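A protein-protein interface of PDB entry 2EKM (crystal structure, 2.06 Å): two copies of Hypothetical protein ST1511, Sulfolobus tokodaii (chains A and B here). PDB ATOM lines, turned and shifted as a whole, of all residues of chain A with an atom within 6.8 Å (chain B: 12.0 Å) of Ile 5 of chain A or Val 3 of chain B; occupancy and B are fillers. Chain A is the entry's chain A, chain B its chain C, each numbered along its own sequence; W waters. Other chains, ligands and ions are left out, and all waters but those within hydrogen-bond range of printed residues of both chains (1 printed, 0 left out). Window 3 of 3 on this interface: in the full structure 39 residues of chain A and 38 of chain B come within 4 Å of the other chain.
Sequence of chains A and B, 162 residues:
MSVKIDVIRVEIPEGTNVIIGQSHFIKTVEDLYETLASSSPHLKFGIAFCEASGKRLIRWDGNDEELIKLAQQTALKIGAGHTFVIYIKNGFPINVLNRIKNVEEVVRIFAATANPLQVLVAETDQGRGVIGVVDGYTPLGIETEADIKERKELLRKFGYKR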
ATOM      1  N   VAL A   3       3.214 -10.166 -23.094  1.00  0.00           N
ATOM      2  CA  VAL A   3       2.963  -8.998 -23.991  1.00  0.00           C
ATOM      3  C   VAL A   3       2.523  -7.767 -23.204  1.00  0.00           C
ATOM      4  O   VAL A   3       1.457  -7.758 -22.587  1.00  0.00           O
ATOM      5  CB  VAL A   3       1.873  -9.322 -25.043  1.00  0.00           C
ATOM      6  CG1 VAL A   3       1.461  -8.053 -25.772  1.00  0.00           C
ATOM      7  CG2 VAL A   3       2.396 -10.346 -26.038  1.00  0.00           C
ATOM      8  N   LYS A   4       3.348  -6.728 -23.236  1.00  0.00           N
ATOM      9  CA  LYS A   4       3.042  -5.489 -22.538  1.00  0.00           C
ATOM     10  C   LYS A   4       2.302  -4.533 -23.470  1.00  0.00           C
ATOM     11  O   LYS A   4       2.561  -4.505 -24.674  1.00  0.00           O
ATOM     12  CB  LYS A   4       4.330  -4.825 -22.057  1.00  0.00           C
ATOM     13  CG  LYS A   4       4.104  -3.496 -21.359  1.00  0.00           C
ATOM     14  CD  LYS A   4       5.416  -2.813 -21.020  1.00  0.00           C
ATOM     15  CE  LYS A   4       5.172  -1.464 -20.360  1.00  0.00           C
ATOM     16  NZ  LYS A   4       6.444  -0.747 -20.078  1.00  0.00           N
ATOM     17  N   ILE A   5       1.382  -3.754 -22.912  1.00  0.00           N
ATOM     18  CA  ILE A   5       0.627  -2.794 -23.705  1.00  0.00           C
ATOM     19  C   ILE A   5       0.836  -1.378 -23.180  1.00  0.00           C
ATOM     20  O   ILE A   5       0.643  -1.108 -21.995  1.00  0.00           O
ATOM     21  CB  ILE A   5      -0.886  -3.111 -23.696  1.00  0.00           C
ATOM     22  CG1 ILE A   5      -1.136  -4.476 -24.344  1.00  0.00           C
ATOM     23  CG2 ILE A   5      -1.651  -2.023 -24.450  1.00  0.00           C
ATOM     24  CD1 ILE A   5      -2.602  -4.885 -24.366  1.00  0.00           C
ATOM     25  N   ASP A   6       1.243  -0.484 -24.073  1.00  0.00           N
ATOM     26  CA  ASP A   6       1.481   0.915 -23.728  1.00  0.00           C
ATOM     27  C   ASP A   6       0.385   1.793 -24.314  1.00  0.00           C
ATOM     28  O   ASP A   6      -0.152   1.500 -25.384  1.00  0.00           O
ATOM     29  CB  ASP A   6       2.835   1.373 -24.275  1.00  0.00           C
ATOM     30  CG  ASP A   6       4.004   0.738 -23.548  1.00  0.00           C
ATOM     31  OD1 ASP A   6       3.800   0.197 -22.443  1.00  0.00           O
ATOM     32  OD2 ASP A   6       5.132   0.789 -24.077  1.00  0.00           O
ATOM     33  N   VAL A   7       0.049   2.861 -23.600  1.00  0.00           N
ATOM     34  CA  VAL A   7      -0.970   3.803 -24.047  1.00  0.00           C
ATOM     35  C   VAL A   7      -0.244   5.093 -24.399  1.00  0.00           C
ATOM     36  O   VAL A   7       0.242   5.795 -23.517  1.00  0.00           O
ATOM     37  CB  VAL A   7      -2.000   4.091 -22.935  1.00  0.00           C
ATOM     38  CG1 VAL A   7      -3.071   5.049 -23.449  1.00  0.00           C
ATOM     39  CG2 VAL A   7      -2.625   2.781 -22.457  1.00  0.00           C
ATOM     40  N   LEU A 120      -2.704   2.568 -28.901  1.00  0.00           N
ATOM     41  CA  LEU A 120      -2.400   1.395 -28.094  1.00  0.00           C
ATOM     42  C   LEU A 120      -1.299   0.600 -28.779  1.00  0.00           C
ATOM     43  O   LEU A 120      -1.470   0.118 -29.898  1.00  0.00           O
ATOM     44  CB  LEU A 120      -3.663   0.544 -27.929  1.00  0.00           C
ATOM     45  CG  LEU A 120      -4.865   1.318 -27.367  1.00  0.00           C
ATOM     46  CD1 LEU A 120      -6.117   0.468 -27.446  1.00  0.00           C
ATOM     47  CD2 LEU A 120      -4.587   1.741 -25.932  1.00  0.00           C
ATOM     48  N   VAL A 121      -0.170   0.457 -28.094  1.00  0.00           N
ATOM     49  CA  VAL A 121       0.979  -0.241 -28.652  1.00  0.00           C
ATOM     50  C   VAL A 121       1.402  -1.474 -27.859  1.00  0.00           C
ATOM     51  O   VAL A 121       1.677  -1.395 -26.663  1.00  0.00           O
ATOM     52  CB  VAL A 121       2.187   0.719 -28.748  1.00  0.00           C
ATOM     53  CG1 VAL A 121       3.345   0.042 -29.462  1.00  0.00           C
ATOM     54  CG2 VAL A 121       1.776   1.993 -29.467  1.00  0.00           C
ATOM     55  N   ALA A 122       1.445  -2.616 -28.536  1.00  0.00           N
ATOM     56  CA  ALA A 122       1.861  -3.858 -27.901  1.00  0.00           C
ATOM     57  C   ALA A 122       3.363  -3.976 -28.109  1.00  0.00           C
ATOM     58  O   ALA A 122       3.880  -3.618 -29.171  1.00  0.00           O
ATOM     59  CB  ALA A 122       1.149  -5.039 -28.538  1.00  0.00           C
ATOM     60  N   GLU A 123       4.067  -4.468 -27.101  1.00  0.00           N
ATOM     61  CA  GLU A 123       5.510  -4.617 -27.206  1.00  0.00           C
ATOM     62  C   GLU A 123       5.892  -6.073 -26.977  1.00  0.00           C
ATOM     63  O   GLU A 123       5.356  -6.726 -26.083  1.00  0.00           O
ATOM     64  CB  GLU A 123       6.202  -3.711 -26.182  1.00  0.00           C
ATOM     65  CG  GLU A 123       7.694  -3.543 -26.399  1.00  0.00           C
ATOM     66  CD  GLU A 123       8.281  -2.458 -25.516  1.00  0.00           C
ATOM     67  OE1 GLU A 123       8.159  -2.573 -24.274  1.00  0.00           O
ATOM     68  OE2 GLU A 123       8.859  -1.491 -26.066  1.00  0.00           O
ATOM     69  N   ILE A 131      -2.008  -1.923 -31.880  1.00  0.00           N
ATOM     70  CA  ILE A 131      -3.155  -2.819 -31.797  1.00  0.00           C
ATOM     71  C   ILE A 131      -4.490  -2.082 -31.847  1.00  0.00           C
ATOM     72  O   ILE A 131      -5.548  -2.708 -31.894  1.00  0.00           O
ATOM     73  CB  ILE A 131      -3.106  -3.689 -30.518  1.00  0.00           C
ATOM     74  CG1 ILE A 131      -3.201  -2.811 -29.272  1.00  0.00           C
ATOM     75  CG2 ILE A 131      -1.827  -4.511 -30.504  1.00  0.00           C
ATOM     76  CD1 ILE A 131      -3.400  -3.607 -27.992  1.00  0.00           C
ATOM     77  N   VAL B   3      -3.893  -2.139 -19.201  1.00  0.00           N
ATOM     78  CA  VAL B   3      -5.226  -1.738 -19.733  1.00  0.00           C
ATOM     79  C   VAL B   3      -6.172  -2.930 -19.717  1.00  0.00           C
ATOM     80  O   VAL B   3      -5.752  -4.069 -19.910  1.00  0.00           O
ATOM     81  CB  VAL B   3      -5.124  -1.218 -21.185  1.00  0.00           C
ATOM     82  CG1 VAL B   3      -4.013  -0.186 -21.290  1.00  0.00           C
ATOM     83  CG2 VAL B   3      -4.881  -2.372 -22.139  1.00  0.00           C
ATOM     84  N   LYS B   4      -7.453  -2.659 -19.498  1.00  0.00           N
ATOM     85  CA  LYS B   4      -8.461  -3.710 -19.453  1.00  0.00           C
ATOM     86  C   LYS B   4      -8.957  -4.060 -20.853  1.00  0.00           C
ATOM     87  O   LYS B   4      -9.126  -3.183 -21.698  1.00  0.00           O
ATOM     88  CB  LYS B   4      -9.639  -3.258 -18.583  1.00  0.00           C
ATOM     89  CG  LYS B   4     -10.771  -4.259 -18.476  1.00  0.00           C
ATOM     90  CD  LYS B   4     -11.944  -3.641 -17.737  1.00  0.00           C
ATOM     91  CE  LYS B   4     -13.112  -4.602 -17.618  1.00  0.00           C
ATOM     92  NZ  LYS B   4     -14.305  -3.925 -17.033  1.00  0.00           N
ATOM     93  N   ILE B   5      -9.184  -5.346 -21.094  1.00  0.00           N
ATOM     94  CA  ILE B   5      -9.673  -5.798 -22.389  1.00  0.00           C
ATOM     95  C   ILE B   5     -11.005  -6.517 -22.223  1.00  0.00           C
ATOM     96  O   ILE B   5     -11.100  -7.495 -21.484  1.00  0.00           O
ATOM     97  CB  ILE B   5      -8.675  -6.758 -23.070  1.00  0.00           C
ATOM     98  CG1 ILE B   5      -7.363  -6.023 -23.364  1.00  0.00           C
ATOM     99  CG2 ILE B   5      -9.278  -7.306 -24.361  1.00  0.00           C
ATOM    100  CD1 ILE B   5      -6.324  -6.869 -24.080  1.00  0.00           C
ATOM    101  N   ASP B   6     -12.034  -6.022 -22.907  1.00  0.00           N
ATOM    102  CA  ASP B   6     -13.356  -6.631 -22.835  1.00  0.00           C
ATOM    103  C   ASP B   6     -13.683  -7.377 -24.117  1.00  0.00           C
ATOM    104  O   ASP B   6     -13.241  -6.997 -25.202  1.00  0.00           O
ATOM    105  CB  ASP B   6     -14.432  -5.572 -22.596  1.00  0.00           C
ATOM    106  CG  ASP B   6     -14.200  -4.789 -21.328  1.00  0.00           C
ATOM    107  OD1 ASP B   6     -13.985  -5.418 -20.271  1.00  0.00           O
ATOM    108  OD2 ASP B   6     -14.239  -3.543 -21.389  1.00  0.00           O
ATOM    109  N   VAL B   7     -14.453  -8.448 -23.978  1.00  0.00           N
ATOM    110  CA  VAL B   7     -14.874  -9.251 -25.115  1.00  0.00           C
ATOM    111  C   VAL B   7     -16.368  -8.997 -25.269  1.00  0.00           C
ATOM    112  O   VAL B   7     -17.162  -9.377 -24.408  1.00  0.00           O
ATOM    113  CB  VAL B   7     -14.616 -10.753 -24.867  1.00  0.00           C
ATOM    114  CG1 VAL B   7     -15.039 -11.569 -26.084  1.00  0.00           C
ATOM    115  CG2 VAL B   7     -13.136 -10.978 -24.567  1.00  0.00           C
ATOM    116  N   LEU B 120     -13.164  -7.162 -29.617  1.00  0.00           N
ATOM    117  CA  LEU B 120     -12.212  -6.942 -28.535  1.00  0.00           C
ATOM    118  C   LEU B 120     -12.045  -5.445 -28.325  1.00  0.00           C
ATOM    119  O   LEU B 120     -11.634  -4.721 -29.234  1.00  0.00           O
ATOM    120  CB  LEU B 120     -10.874  -7.594 -28.880  1.00  0.00           C
ATOM    121  CG  LEU B 120     -11.001  -9.068 -29.284  1.00  0.00           C
ATOM    122  CD1 LEU B 120      -9.626  -9.644 -29.564  1.00  0.00           C
ATOM    123  CD2 LEU B 120     -11.693  -9.850 -28.174  1.00  0.00           C
ATOM    124  N   VAL B 121     -12.364  -4.993 -27.118  1.00  0.00           N
ATOM    125  CA  VAL B 121     -12.303  -3.579 -26.780  1.00  0.00           C
ATOM    126  C   VAL B 121     -11.365  -3.270 -25.617  1.00  0.00           C
ATOM    127  O   VAL B 121     -11.505  -3.827 -24.527  1.00  0.00           O
ATOM    128  CB  VAL B 121     -13.707  -3.062 -26.397  1.00  0.00           C
ATOM    129  CG1 VAL B 121     -13.660  -1.568 -26.111  1.00  0.00           C
ATOM    130  CG2 VAL B 121     -14.698  -3.390 -27.497  1.00  0.00           C
ATOM    131  N   ALA B 122     -10.412  -2.374 -25.853  1.00  0.00           N
ATOM    132  CA  ALA B 122      -9.482  -1.972 -24.808  1.00  0.00           C
ATOM    133  C   ALA B 122     -10.076  -0.744 -24.127  1.00  0.00           C
ATOM    134  O   ALA B 122     -10.692   0.097 -24.785  1.00  0.00           O
ATOM    135  CB  ALA B 122      -8.114  -1.631 -25.412  1.00  0.00           C
ATOM    136  N   GLU B 123      -9.903  -0.644 -22.815  1.00  0.00           N
ATOM    137  CA  GLU B 123     -10.430   0.497 -22.078  1.00  0.00           C
ATOM    138  C   GLU B 123      -9.305   1.184 -21.324  1.00  0.00           C
ATOM    139  O   GLU B 123      -8.541   0.533 -20.619  1.00  0.00           O
ATOM    140  CB  GLU B 123     -11.509   0.041 -21.098  1.00  0.00           C
ATOM    141  CG  GLU B 123     -12.247   1.182 -20.414  1.00  0.00           C
ATOM    142  CD  GLU B 123     -13.483   0.704 -19.680  1.00  0.00           C
ATOM    143  OE1 GLU B 123     -13.332  -0.066 -18.703  1.00  0.00           O
ATOM    144  OE2 GLU B 123     -14.600   1.092 -20.088  1.00  0.00           O
ATOM    145  N   THR B 124      -9.196   2.499 -21.492  1.00  0.00           N
ATOM    146  CA  THR B 124      -8.160   3.273 -20.822  1.00  0.00           C
ATOM    147  C   THR B 124      -8.825   4.342 -19.969  1.00  0.00           C
ATOM    148  O   THR B 124     -10.048   4.358 -19.818  1.00  0.00           O
ATOM    149  CB  THR B 124      -7.241   3.989 -21.828  1.00  0.00           C
ATOM    150  OG1 THR B 124      -7.999   4.983 -22.530  1.00  0.00           O
ATOM    151  CG2 THR B 124      -6.665   2.993 -22.833  1.00  0.00           C
ATOM    152  N   ASP B 125      -8.018   5.248 -19.426  1.00  0.00           N
ATOM    153  CA  ASP B 125      -8.543   6.326 -18.599  1.00  0.00           C
ATOM    154  C   ASP B 125      -9.344   7.323 -19.442  1.00  0.00           C
ATOM    155  O   ASP B 125     -10.173   8.065 -18.919  1.00  0.00           O
ATOM    156  CB  ASP B 125      -7.396   7.034 -17.866  1.00  0.00           C
ATOM    157  CG  ASP B 125      -6.322   7.563 -18.812  1.00  0.00           C
ATOM    158  OD1 ASP B 125      -6.327   7.209 -20.009  1.00  0.00           O
ATOM    159  OD2 ASP B 125      -5.459   8.333 -18.346  1.00  0.00           O
ATOM    160  N   GLN B 126      -9.111   7.326 -20.751  1.00  0.00           N
ATOM    161  CA  GLN B 126      -9.831   8.239 -21.635  1.00  0.00           C
ATOM    162  C   GLN B 126     -11.132   7.644 -22.160  1.00  0.00           C
ATOM    163  O   GLN B 126     -12.180   8.285 -22.119  1.00  0.00           O
ATOM    164  CB  GLN B 126      -8.964   8.636 -22.830  1.00  0.00           C
ATOM    165  CG  GLN B 126      -9.669   9.570 -23.803  1.00  0.00           C
ATOM    166  CD  GLN B 126      -8.819   9.891 -25.018  1.00  0.00           C
ATOM    167  OE1 GLN B 126      -7.674  10.323 -24.890  1.00  0.00           O
ATOM    168  NE2 GLN B 126      -9.379   9.684 -26.206  1.00  0.00           N
ATOM    169  N   GLY B 127     -11.059   6.422 -22.672  1.00  0.00           N
ATOM    170  CA  GLY B 127     -12.252   5.794 -23.210  1.00  0.00           C
ATOM    171  C   GLY B 127     -12.023   4.370 -23.660  1.00  0.00           C
ATOM    172  O   GLY B 127     -11.227   3.648 -23.065  1.00  0.00           O
ATOM    173  N   ARG B 128     -12.720   3.972 -24.722  1.00  0.00           N
ATOM    174  CA  ARG B 128     -12.618   2.622 -25.256  1.00  0.00           C
ATOM    175  C   ARG B 128     -12.151   2.626 -26.716  1.00  0.00           C
ATOM    176  O   ARG B 128     -12.416   3.568 -27.463  1.00  0.00           O
ATOM    177  CB  ARG B 128     -13.981   1.922 -25.135  1.00  0.00           C
ATOM    178  CG  ARG B 128     -14.460   1.751 -23.684  1.00  0.00           C
ATOM    179  CD  ARG B 128     -15.966   1.491 -23.592  1.00  0.00           C
ATOM    180  NE  ARG B 128     -16.368   0.207 -24.166  1.00  0.00           N
ATOM    181  CZ  ARG B 128     -16.282  -0.963 -23.537  1.00  0.00           C
ATOM    182  NH1 ARG B 128     -15.809  -1.022 -22.300  1.00  0.00           N
ATOM    183  NH2 ARG B 128     -16.667  -2.078 -24.147  1.00  0.00           N
ATOM    184  N   GLY B 129     -11.438   1.573 -27.102  1.00  0.00           N
ATOM    185  CA  GLY B 129     -10.947   1.454 -28.465  1.00  0.00           C
ATOM    186  C   GLY B 129     -10.971   0.000 -28.907  1.00  0.00           C
ATOM    187  O   GLY B 129     -10.689  -0.894 -28.109  1.00  0.00           O
ATOM    188  N   VAL B 130     -11.314  -0.240 -30.170  1.00  0.00           N
ATOM    189  CA  VAL B 130     -11.376  -1.599 -30.704  1.00  0.00           C
ATOM    190  C   VAL B 130      -9.984  -2.080 -31.103  1.00  0.00           C
ATOM    191  O   VAL B 130      -9.294  -1.413 -31.868  1.00  0.00           O
ATOM    192  CB  VAL B 130     -12.302  -1.661 -31.949  1.00  0.00           C
ATOM    193  CG1 VAL B 130     -12.329  -3.071 -32.516  1.00  0.00           C
ATOM    194  CG2 VAL B 130     -13.712  -1.208 -31.573  1.00  0.00           C
ATOM    195  N   ILE B 131      -9.568  -3.235 -30.583  1.00  0.00           N
ATOM    196  CA  ILE B 131      -8.252  -3.776 -30.918  1.00  0.00           C
ATOM    197  C   ILE B 131      -8.350  -4.982 -31.845  1.00  0.00           C
ATOM    198  O   ILE B 131      -7.334  -5.514 -32.287  1.00  0.00           O
ATOM    199  CB  ILE B 131      -7.444  -4.190 -29.652  1.00  0.00           C
ATOM    200  CG1 ILE B 131      -8.173  -5.301 -28.893  1.00  0.00           C
ATOM    201  CG2 ILE B 131      -7.210  -2.973 -28.757  1.00  0.00           C
ATOM    202  CD1 ILE B 131      -7.354  -5.882 -27.744  1.00  0.00           C
ATOM    203  N   GLY B 132      -9.573  -5.415 -32.131  1.00  0.00           N
ATOM    204  CA  GLY B 132      -9.750  -6.551 -33.016  1.00  0.00           C
ATOM    205  C   GLY B 132     -11.066  -7.275 -32.817  1.00  0.00           C
ATOM    206  O   GLY B 132     -11.899  -6.867 -32.005  1.00  0.00           O
HETATM  207  O   HOH W   1      -7.305  -2.217 -34.055  1.00  0.00           O
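The backbone carbonyl oxygen (O) of Ile 131 of chain A lies close to the backbone carbonyl oxygen (O) of Ile 131 of chain B.
N of Ile 131 of chain A lies within hydrogen-bond range of O of Leu 120 of chain A (2.9 Å).
O of Leu 120 of chain B is in hydrogen-bond range of N of Ile 131 of chain B, 2.9 Å away.
The backbone NH (N) of Ala 122 of chain B is in hydrogen-bond range of the backbone carbonyl oxygen (O) of Gly 129 of chain B (2.7 Å).
The backbone NH (N) of Gln 126 of chain B sits close to the side-chain hydroxyl (OG1) of Thr 124 of chain B (3.1 Å).
The backbone NH of Gly 127 of chain B is in hydrogen-bond range of the side-chain hydroxyl of Thr 124 of chain B.
Ile 5 of chain A touches Val 3 of chain B.
CG1 of Val 3 of chain B touches CG2 of Val 7 of chain A, at 3.5 Å.
CB of Ala 122 of chain B touches CD1 of Leu 120 of chain A (3.5 Å).
Leu 120 of chain A touches Thr 124 of chain B.
CD1 of Leu 120 of chain A touches CG2 of Ile 131 of chain B, 3.8 Å away.
Val 130 of chain B touches Ile 131 of chain A.
No residue of chain B comes within 4 Å of Lys 4 of chain A.
Printed residues of chain B within 4 Å of Ile 5 of chain A: Val 3 (3.99 Å).
Leu 120 of chain A touches three residues of chain B.
No residue of chain B comes within 4 Å of Val 121 of chain A.
No residue of chain B comes within 4 Å of Ala 122 of chain A.
Printed residues of chain B within 4 Å of Ile 131 of chain A: Val 130 and Ile 131.
Of the printed residues of chain A, Val 3 of chain B touches Ile 5 (3.99 Å) and Val 7 (3.5 Å).
Of the printed residues of chain A, Ala 122 of chain B touches Leu 120.
Of the printed residues of chain A, Val 130 of chain B touches Ile 131 (3.96 Å).
Printed residues of chain A within 4 Å of Ile 131 of chain B: Leu 120 and Ile 131.
The nearest printed residue of chain B that does not touch Ile 131 of chain A is Gly 132 of chain B (4.9 Å).
Hydrophobic or aromatic side chains of chain B within 4 Å of the printed part of chain A: Val 3, Ala 122 and Ile 131.
Hydrophobic or aromatic side chains of chain A that line the printed part of chain B: Ile 5, Val 7, Leu 120 and Ile 131.
Among the printed residues, 7 pairs touch across the chains.
Among the printed residues, no Asp or Glu carboxylate lies within 4 Å of a Lys or Arg side-chain nitrogen of the other chain.
Ile 5 of chain A touches Val 3 of chain B, but with the chains exchanged Val 3 of chain A does not touch Ile 5 of chain B (8.0 Å).
Leu 120 of chain A touches Ala 122 of chain B, but with the chains exchanged Ala 122 of chain A does not touch Leu 120 of chain B (11.8 Å).
Leu 120 of chain A touches Ile 131 of chain B, but with the chains exchanged Ile 131 of chain A does not touch Leu 120 of chain B (6.9 Å).
Ile 131 of chain A touches its own counterpart, Ile 131 of chain B.
Positions printed for both chains: 3, 4, 5, 6, 7, 120, 121, 122, 123 and 131.
Water W1 bridges the backbone carbonyl oxygen (O) of Ile 131 of chain A (2.8 Å) and the backbone carbonyl oxygen (O) of Val 130 of chain B (3.1 Å).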
